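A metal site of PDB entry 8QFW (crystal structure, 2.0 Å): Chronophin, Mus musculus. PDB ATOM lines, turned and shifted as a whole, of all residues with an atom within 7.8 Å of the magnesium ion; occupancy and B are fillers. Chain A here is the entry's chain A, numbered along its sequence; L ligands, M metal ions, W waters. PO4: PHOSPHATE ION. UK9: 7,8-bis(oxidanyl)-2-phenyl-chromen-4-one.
O4 of PO4 L1 is bound to the magnesium ion (2.0 Å).
Water W1 is bound to the magnesium ion (2.1 Å).
OD1 of Asp 235 binds the magnesium ion (2.1 Å).
The magnesium ion is bound by water W2, 2.2 Å away.
The side-chain carboxylate (OD2) of Asp 26 is bound to the magnesium ion, at 2.2 Å.
The magnesium ion is bound by the backbone carbonyl oxygen (O) of Asp 28 (2.2 Å).
Asp 240 touches the magnesium ion (OD2 to MG, 3.9 Å).
Four residues have an atom within 4 Å of the magnesium ion: Asp 26, Asp 28, Asp 235 and Asp 240.
The backbone NH of Asp 235 sits at hydrogen-bond distance from the side-chain carboxylate of Asp 240, 3.1 Å away.
The side-chain carboxylate (OD2) of Asp 235 lies within hydrogen-bond range of the backbone NH (N) of Val 258 (2.9 Å).
OD1 of Asp 26 lies within salt-bridge range of NZ of Lys 210.
The backbone NH (N) of Asp 26 sits at hydrogen-bond distance from the backbone carbonyl oxygen (O) of Val 233 (2.9 Å).
OD1 of Asp 28 sits at hydrogen-bond distance from NE1 of Trp 32 (2.8 Å).
NZ of Lys 210 is in salt-bridge range of OD1 of Asp 240, at 2.7 Å.
N of Arg 236 sits at hydrogen-bond distance from OD2 of Asp 240, 3.1 Å away.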
ATOM      1  N   ASP A  26      -0.112  23.960   2.617  1.00  0.00           N
ATOM      2  CA  ASP A  26       0.599  22.692   2.686  1.00  0.00           C
ATOM      3  C   ASP A  26       1.073  22.316   1.285  1.00  0.00           C
ATOM      4  O   ASP A  26       0.525  22.780   0.278  1.00  0.00           O
ATOM      5  CB  ASP A  26      -0.290  21.603   3.278  1.00  0.00           C
ATOM      6  CG  ASP A  26       0.382  20.234   3.264  1.00  0.00           C
ATOM      7  OD1 ASP A  26       1.463  20.089   3.871  1.00  0.00           O
ATOM      8  OD2 ASP A  26      -0.181  19.315   2.625  1.00  0.00           O
ATOM      9  N   CYS A  27       2.103  21.485   1.221  1.00  0.00           N
ATOM     10  CA  CYS A  27       2.732  21.182  -0.061  1.00  0.00           C
ATOM     11  C   CYS A  27       2.259  19.861  -0.664  1.00  0.00           C
ATOM     12  O   CYS A  27       1.536  19.869  -1.665  1.00  0.00           O
ATOM     13  CB  CYS A  27       4.258  21.179   0.095  1.00  0.00           C
ATOM     14  SG  CYS A  27       4.952  22.806   0.499  1.00  0.00           S
ATOM     15  N   ASP A  28       2.651  18.738  -0.067  1.00  0.00           N
ATOM     16  CA  ASP A  28       2.317  17.441  -0.641  1.00  0.00           C
ATOM     17  C   ASP A  28       0.809  17.208  -0.628  1.00  0.00           C
ATOM     18  O   ASP A  28       0.153  17.391   0.409  1.00  0.00           O
ATOM     19  CB  ASP A  28       3.035  16.315   0.106  1.00  0.00           C
ATOM     20  CG  ASP A  28       4.548  16.439   0.035  1.00  0.00           C
ATOM     21  OD1 ASP A  28       5.062  16.874  -1.011  1.00  0.00           O
ATOM     22  OD2 ASP A  28       5.211  16.104   1.032  1.00  0.00           O
ATOM     23  N   GLY A  29       0.259  16.808  -1.771  1.00  0.00           N
ATOM     24  CA  GLY A  29      -1.159  16.604  -1.911  1.00  0.00           C
ATOM     25  C   GLY A  29      -1.954  17.867  -2.155  1.00  0.00           C
ATOM     26  O   GLY A  29      -3.176  17.790  -2.333  1.00  0.00           O
ATOM     27  N   VAL A  30      -1.294  19.026  -2.189  1.00  0.00           N
ATOM     28  CA  VAL A  30      -1.959  20.320  -2.334  1.00  0.00           C
ATOM     29  C   VAL A  30      -1.422  21.000  -3.578  1.00  0.00           C
ATOM     30  O   VAL A  30      -2.190  21.346  -4.490  1.00  0.00           O
ATOM     31  CB  VAL A  30      -1.735  21.186  -1.073  1.00  0.00           C
ATOM     32  CG1 VAL A  30      -2.299  22.578  -1.275  1.00  0.00           C
ATOM     33  CG2 VAL A  30      -2.355  20.516   0.142  1.00  0.00           C
ATOM     34  N   LEU A  31      -0.106  21.218  -3.621  1.00  0.00           N
ATOM     35  CA  LEU A  31       0.536  21.792  -4.794  1.00  0.00           C
ATOM     36  C   LEU A  31       0.961  20.754  -5.808  1.00  0.00           C
ATOM     37  O   LEU A  31       1.117  21.082  -6.993  1.00  0.00           O
ATOM     38  CB  LEU A  31       1.777  22.595  -4.376  1.00  0.00           C
ATOM     39  CG  LEU A  31       1.594  23.690  -3.321  1.00  0.00           C
ATOM     40  CD1 LEU A  31       2.950  24.227  -2.899  1.00  0.00           C
ATOM     41  CD2 LEU A  31       0.709  24.798  -3.847  1.00  0.00           C
ATOM     42  N   TRP A  32       1.166  19.514  -5.386  1.00  0.00           N
ATOM     43  CA  TRP A  32       1.704  18.473  -6.245  1.00  0.00           C
ATOM     44  C   TRP A  32       1.509  17.128  -5.579  1.00  0.00           C
ATOM     45  O   TRP A  32       1.273  17.040  -4.364  1.00  0.00           O
ATOM     46  CB  TRP A  32       3.187  18.707  -6.539  1.00  0.00           C
ATOM     47  CG  TRP A  32       4.040  18.836  -5.301  1.00  0.00           C
ATOM     48  CD1 TRP A  32       4.219  17.882  -4.332  1.00  0.00           C
ATOM     49  CD2 TRP A  32       4.817  19.966  -4.906  1.00  0.00           C
ATOM     50  NE1 TRP A  32       5.059  18.357  -3.361  1.00  0.00           N
ATOM     51  CE2 TRP A  32       5.447  19.633  -3.683  1.00  0.00           C
ATOM     52  CE3 TRP A  32       5.053  21.228  -5.460  1.00  0.00           C
ATOM     53  CZ2 TRP A  32       6.285  20.525  -3.018  1.00  0.00           C
ATOM     54  CZ3 TRP A  32       5.881  22.098  -4.801  1.00  0.00           C
ATOM     55  CH2 TRP A  32       6.495  21.744  -3.592  1.00  0.00           C
ATOM     56  N   ASN A  33       1.629  16.075  -6.385  1.00  0.00           N
ATOM     57  CA  ASN A  33       1.748  14.704  -5.896  1.00  0.00           C
ATOM     58  C   ASN A  33       2.914  14.073  -6.648  1.00  0.00           C
ATOM     59  O   ASN A  33       2.804  13.814  -7.855  1.00  0.00           O
ATOM     60  CB  ASN A  33       0.457  13.914  -6.098  1.00  0.00           C
ATOM     61  CG  ASN A  33      -0.652  14.355  -5.157  1.00  0.00           C
ATOM     62  OD1 ASN A  33      -0.578  14.128  -3.948  1.00  0.00           O
ATOM     63  ND2 ASN A  33      -1.700  14.965  -5.706  1.00  0.00           N
ATOM     64  N   VAL A  58       4.052  25.238   4.268  1.00  0.00           N
ATOM     65  CA  VAL A  58       4.419  24.287   5.301  1.00  0.00           C
ATOM     66  C   VAL A  58       4.402  22.877   4.715  1.00  0.00           C
ATOM     67  O   VAL A  58       3.704  22.601   3.740  1.00  0.00           O
ATOM     68  CB  VAL A  58       3.482  24.359   6.529  1.00  0.00           C
ATOM     69  CG1 VAL A  58       3.857  25.528   7.416  1.00  0.00           C
ATOM     70  CG2 VAL A  58       2.019  24.451   6.092  1.00  0.00           C
ATOM     71  N   SER A  59       5.193  22.003   5.315  1.00  0.00           N
ATOM     72  CA  SER A  59       5.273  20.610   4.877  1.00  0.00           C
ATOM     73  C   SER A  59       5.918  19.798   5.990  1.00  0.00           C
ATOM     74  O   SER A  59       6.903  20.231   6.580  1.00  0.00           O
ATOM     75  CB  SER A  59       6.066  20.472   3.578  1.00  0.00           C
ATOM     76  OG  SER A  59       6.086  19.116   3.149  1.00  0.00           O
ATOM     77  N   ASN A  60       5.350  18.631   6.276  1.00  0.00           N
ATOM     78  CA  ASN A  60       5.999  17.694   7.184  1.00  0.00           C
ATOM     79  C   ASN A  60       7.038  16.832   6.477  1.00  0.00           C
ATOM     80  O   ASN A  60       7.710  16.028   7.136  1.00  0.00           O
ATOM     81  CB  ASN A  60       4.948  16.823   7.878  1.00  0.00           C
ATOM     82  CG  ASN A  60       4.223  17.566   8.973  1.00  0.00           C
ATOM     83  OD1 ASN A  60       4.695  18.598   9.468  1.00  0.00           O
ATOM     84  ND2 ASN A  60       3.059  17.058   9.375  1.00  0.00           N
ATOM     85  N   ASP A 176       2.761  12.198  11.241  1.00  0.00           N
ATOM     86  CA  ASP A 176       2.022  11.648  10.114  1.00  0.00           C
ATOM     87  C   ASP A 176       2.147  10.129  10.117  1.00  0.00           C
ATOM     88  O   ASP A 176       3.276   9.610  10.132  1.00  0.00           O
ATOM     89  CB  ASP A 176       2.529  12.218   8.792  1.00  0.00           C
ATOM     90  CG  ASP A 176       2.216  13.683   8.619  1.00  0.00           C
ATOM     91  OD1 ASP A 176       1.631  14.276   9.553  1.00  0.00           O
ATOM     92  OD2 ASP A 176       2.527  14.238   7.550  1.00  0.00           O
ATOM     93  N   HIS A 179       2.205   7.813   4.295  1.00  0.00           N
ATOM     94  CA  HIS A 179       2.180   8.710   3.156  1.00  0.00           C
ATOM     95  C   HIS A 179       1.891   7.930   1.883  1.00  0.00           C
ATOM     96  O   HIS A 179       2.409   6.818   1.701  1.00  0.00           O
ATOM     97  CB  HIS A 179       3.516   9.454   3.014  1.00  0.00           C
ATOM     98  CG  HIS A 179       3.838  10.345   4.172  1.00  0.00           C
ATOM     99  ND1 HIS A 179       3.184  11.542   4.389  1.00  0.00           N
ATOM    100  CD2 HIS A 179       4.722  10.211   5.182  1.00  0.00           C
ATOM    101  CE1 HIS A 179       3.666  12.104   5.484  1.00  0.00           C
ATOM    102  NE2 HIS A 179       4.603  11.323   5.978  1.00  0.00           N
ATOM    103  N   PRO A 180       1.074   8.478   0.979  1.00  0.00           N
ATOM    104  CA  PRO A 180       0.810   7.777  -0.286  1.00  0.00           C
ATOM    105  C   PRO A 180       1.925   8.008  -1.286  1.00  0.00           C
ATOM    106  O   PRO A 180       2.551   9.066  -1.335  1.00  0.00           O
ATOM    107  CB  PRO A 180      -0.501   8.416  -0.757  1.00  0.00           C
ATOM    108  CG  PRO A 180      -0.402   9.821  -0.260  1.00  0.00           C
ATOM    109  CD  PRO A 180       0.324   9.747   1.069  1.00  0.00           C
ATOM    110  N   LYS A 210       3.237  20.361  12.053  1.00  0.00           N
ATOM    111  CA  LYS A 210       1.780  20.425  12.151  1.00  0.00           C
ATOM    112  C   LYS A 210       1.218  19.029  12.415  1.00  0.00           C
ATOM    113  O   LYS A 210       1.725  18.041  11.857  1.00  0.00           O
ATOM    114  CB  LYS A 210       1.195  21.000  10.854  1.00  0.00           C
ATOM    115  CG  LYS A 210       1.660  20.321   9.573  1.00  0.00           C
ATOM    116  CD  LYS A 210       1.314  21.168   8.349  1.00  0.00           C
ATOM    117  CE  LYS A 210       1.837  20.551   7.054  1.00  0.00           C
ATOM    118  NZ  LYS A 210       1.313  19.177   6.795  1.00  0.00           N
ATOM    119  N   VAL A 233      -4.597  26.050   3.920  1.00  0.00           N
ATOM    120  CA  VAL A 233      -5.029  25.156   2.849  1.00  0.00           C
ATOM    121  C   VAL A 233      -4.213  23.875   2.937  1.00  0.00           C
ATOM    122  O   VAL A 233      -2.983  23.907   2.840  1.00  0.00           O
ATOM    123  CB  VAL A 233      -4.876  25.809   1.472  1.00  0.00           C
ATOM    124  CG1 VAL A 233      -5.400  24.878   0.380  1.00  0.00           C
ATOM    125  CG2 VAL A 233      -5.598  27.150   1.434  1.00  0.00           C
ATOM    126  N   GLY A 234      -4.904  22.744   3.123  1.00  0.00           N
ATOM    127  CA  GLY A 234      -4.235  21.468   3.252  1.00  0.00           C
ATOM    128  C   GLY A 234      -5.127  20.337   2.774  1.00  0.00           C
ATOM    129  O   GLY A 234      -6.312  20.533   2.487  1.00  0.00           O
ATOM    130  N   ASP A 235      -4.533  19.140   2.709  1.00  0.00           N
ATOM    131  CA  ASP A 235      -5.217  17.960   2.210  1.00  0.00           C
ATOM    132  C   ASP A 235      -5.472  16.901   3.270  1.00  0.00           C
ATOM    133  O   ASP A 235      -6.103  15.882   2.975  1.00  0.00           O
ATOM    134  CB  ASP A 235      -4.409  17.330   1.064  1.00  0.00           C
ATOM    135  CG  ASP A 235      -3.101  16.732   1.541  1.00  0.00           C
ATOM    136  OD1 ASP A 235      -2.295  17.459   2.155  1.00  0.00           O
ATOM    137  OD2 ASP A 235      -2.887  15.524   1.296  1.00  0.00           O
ATOM    138  N   ARG A 236      -4.990  17.093   4.499  1.00  0.00           N
ATOM    139  CA  ARG A 236      -5.061  16.059   5.525  1.00  0.00           C
ATOM    140  C   ARG A 236      -5.788  16.620   6.741  1.00  0.00           C
ATOM    141  O   ARG A 236      -5.311  17.560   7.385  1.00  0.00           O
ATOM    142  CB  ARG A 236      -3.649  15.580   5.885  1.00  0.00           C
ATOM    143  CG  ARG A 236      -3.614  14.188   6.507  1.00  0.00           C
ATOM    144  CD  ARG A 236      -2.238  13.554   6.336  1.00  0.00           C
ATOM    145  NE  ARG A 236      -2.257  12.133   6.648  1.00  0.00           N
ATOM    146  CZ  ARG A 236      -1.315  11.264   6.280  1.00  0.00           C
ATOM    147  NH1 ARG A 236      -0.257  11.654   5.602  1.00  0.00           N
ATOM    148  NH2 ARG A 236      -1.456   9.985   6.600  1.00  0.00           N
ATOM    149  N   THR A 239      -3.922  16.577  10.255  1.00  0.00           N
ATOM    150  CA  THR A 239      -2.727  17.406  10.401  1.00  0.00           C
ATOM    151  C   THR A 239      -2.988  18.849   9.981  1.00  0.00           C
ATOM    152  O   THR A 239      -2.854  19.754  10.799  1.00  0.00           O
ATOM    153  CB  THR A 239      -1.566  16.828   9.585  1.00  0.00           C
ATOM    154  OG1 THR A 239      -1.837  16.952   8.183  1.00  0.00           O
ATOM    155  CG2 THR A 239      -1.348  15.361   9.918  1.00  0.00           C
ATOM    156  N   ASP A 240      -3.375  19.079   8.725  1.00  0.00           N
ATOM    157  CA  ASP A 240      -3.495  20.454   8.221  1.00  0.00           C
ATOM    158  C   ASP A 240      -4.694  21.170   8.824  1.00  0.00           C
ATOM    159  O   ASP A 240      -4.594  22.336   9.230  1.00  0.00           O
ATOM    160  CB  ASP A 240      -3.592  20.434   6.696  1.00  0.00           C
ATOM    161  CG  ASP A 240      -2.396  19.762   6.055  1.00  0.00           C
ATOM    162  OD1 ASP A 240      -1.261  20.009   6.502  1.00  0.00           O
ATOM    163  OD2 ASP A 240      -2.592  18.972   5.107  1.00  0.00           O
ATOM    164  N   THR A 254      -8.488  20.712   0.532  1.00  0.00           N
ATOM    165  CA  THR A 254      -8.443  20.399  -0.889  1.00  0.00           C
ATOM    166  C   THR A 254      -8.454  18.879  -1.048  1.00  0.00           C
ATOM    167  O   THR A 254      -7.849  18.164  -0.252  1.00  0.00           O
ATOM    168  CB  THR A 254      -7.214  21.012  -1.558  1.00  0.00           C
ATOM    169  OG1 THR A 254      -7.255  20.752  -2.970  1.00  0.00           O
ATOM    170  CG2 THR A 254      -5.925  20.458  -0.968  1.00  0.00           C
ATOM    171  N   GLY A 257      -5.550  15.229  -2.314  1.00  0.00           N
ATOM    172  CA  GLY A 257      -4.575  14.541  -1.488  1.00  0.00           C
ATOM    173  C   GLY A 257      -5.122  13.409  -0.648  1.00  0.00           C
ATOM    174  O   GLY A 257      -5.852  12.543  -1.148  1.00  0.00           O
ATOM    175  N   VAL A 258      -4.776  13.408   0.639  1.00  0.00           N
ATOM    176  CA  VAL A 258      -5.035  12.256   1.491  1.00  0.00           C
ATOM    177  C   VAL A 258      -6.502  12.165   1.881  1.00  0.00           C
ATOM    178  O   VAL A 258      -7.153  11.131   1.679  1.00  0.00           O
ATOM    179  CB  VAL A 258      -4.127  12.308   2.737  1.00  0.00           C
ATOM    180  CG1 VAL A 258      -4.562  11.274   3.757  1.00  0.00           C
ATOM    181  CG2 VAL A 258      -2.664  12.116   2.345  1.00  0.00           C
HETATM  182  P   PO4 L   1       3.019  17.324   3.600  1.00  0.00           P
HETATM  183  O1  PO4 L   1       2.908  17.670   5.065  1.00  0.00           O
HETATM  184  O2  PO4 L   1       4.128  16.322   3.424  1.00  0.00           O
HETATM  185  O3  PO4 L   1       3.313  18.567   2.790  1.00  0.00           O
HETATM  186  O4  PO4 L   1       1.702  16.751   3.119  1.00  0.00           O
HETATM  187  C2  UK9 L   2       7.977  11.903   2.336  1.00  0.00           C
HETATM  188  C4  UK9 L   2       6.519  10.715   0.715  1.00  0.00           C
HETATM  189  C6  UK9 L   2       4.311  11.515   0.203  1.00  0.00           C
HETATM  190  C7  UK9 L   2       4.491  12.562   1.086  1.00  0.00           C
HETATM  191  C9  UK9 L   2      10.289  11.373   2.184  1.00  0.00           C
HETATM  192  C11 UK9 L   2      12.601  10.787   1.939  1.00  0.00           C
HETATM  193  C12 UK9 L   2      12.884  11.444   3.122  1.00  0.00           C
HETATM  194  C13 UK9 L   2      11.872  12.070   3.841  1.00  0.00           C
HETATM  195  C14 UK9 L   2      10.564  12.035   3.376  1.00  0.00           C
HETATM  196  C   UK9 L   2       9.463  12.665   4.116  1.00  0.00           C
HETATM  197  O   UK9 L   2       9.634  13.253   5.195  1.00  0.00           O
HETATM  198  O1  UK9 L   2       9.009  11.312   1.657  1.00  0.00           O
HETATM  199  O2  UK9 L   2      11.006  10.108   0.282  1.00  0.00           O
HETATM  200  C1  UK9 L   2       8.161  12.550   3.507  1.00  0.00           C
HETATM  201  C10 UK9 L   2      11.295  10.742   1.442  1.00  0.00           C
HETATM  202  C3  UK9 L   2       6.705  11.761   1.604  1.00  0.00           C
HETATM  203  C5  UK9 L   2       5.329  10.593   0.014  1.00  0.00           C
HETATM  204  C8  UK9 L   2       5.674  12.679   1.793  1.00  0.00           C
HETATM  205  O3  UK9 L   2      13.594  10.176   1.227  1.00  0.00           O
HETATM  206 MG    MG M   1      -0.218  17.144   2.548  1.00  0.00          MG
HETATM  207  O   HOH W   1      -0.723  17.099   4.567  1.00  0.00           O
HETATM  208  O   HOH W   2      -0.395  15.029   2.200  1.00  0.00           O
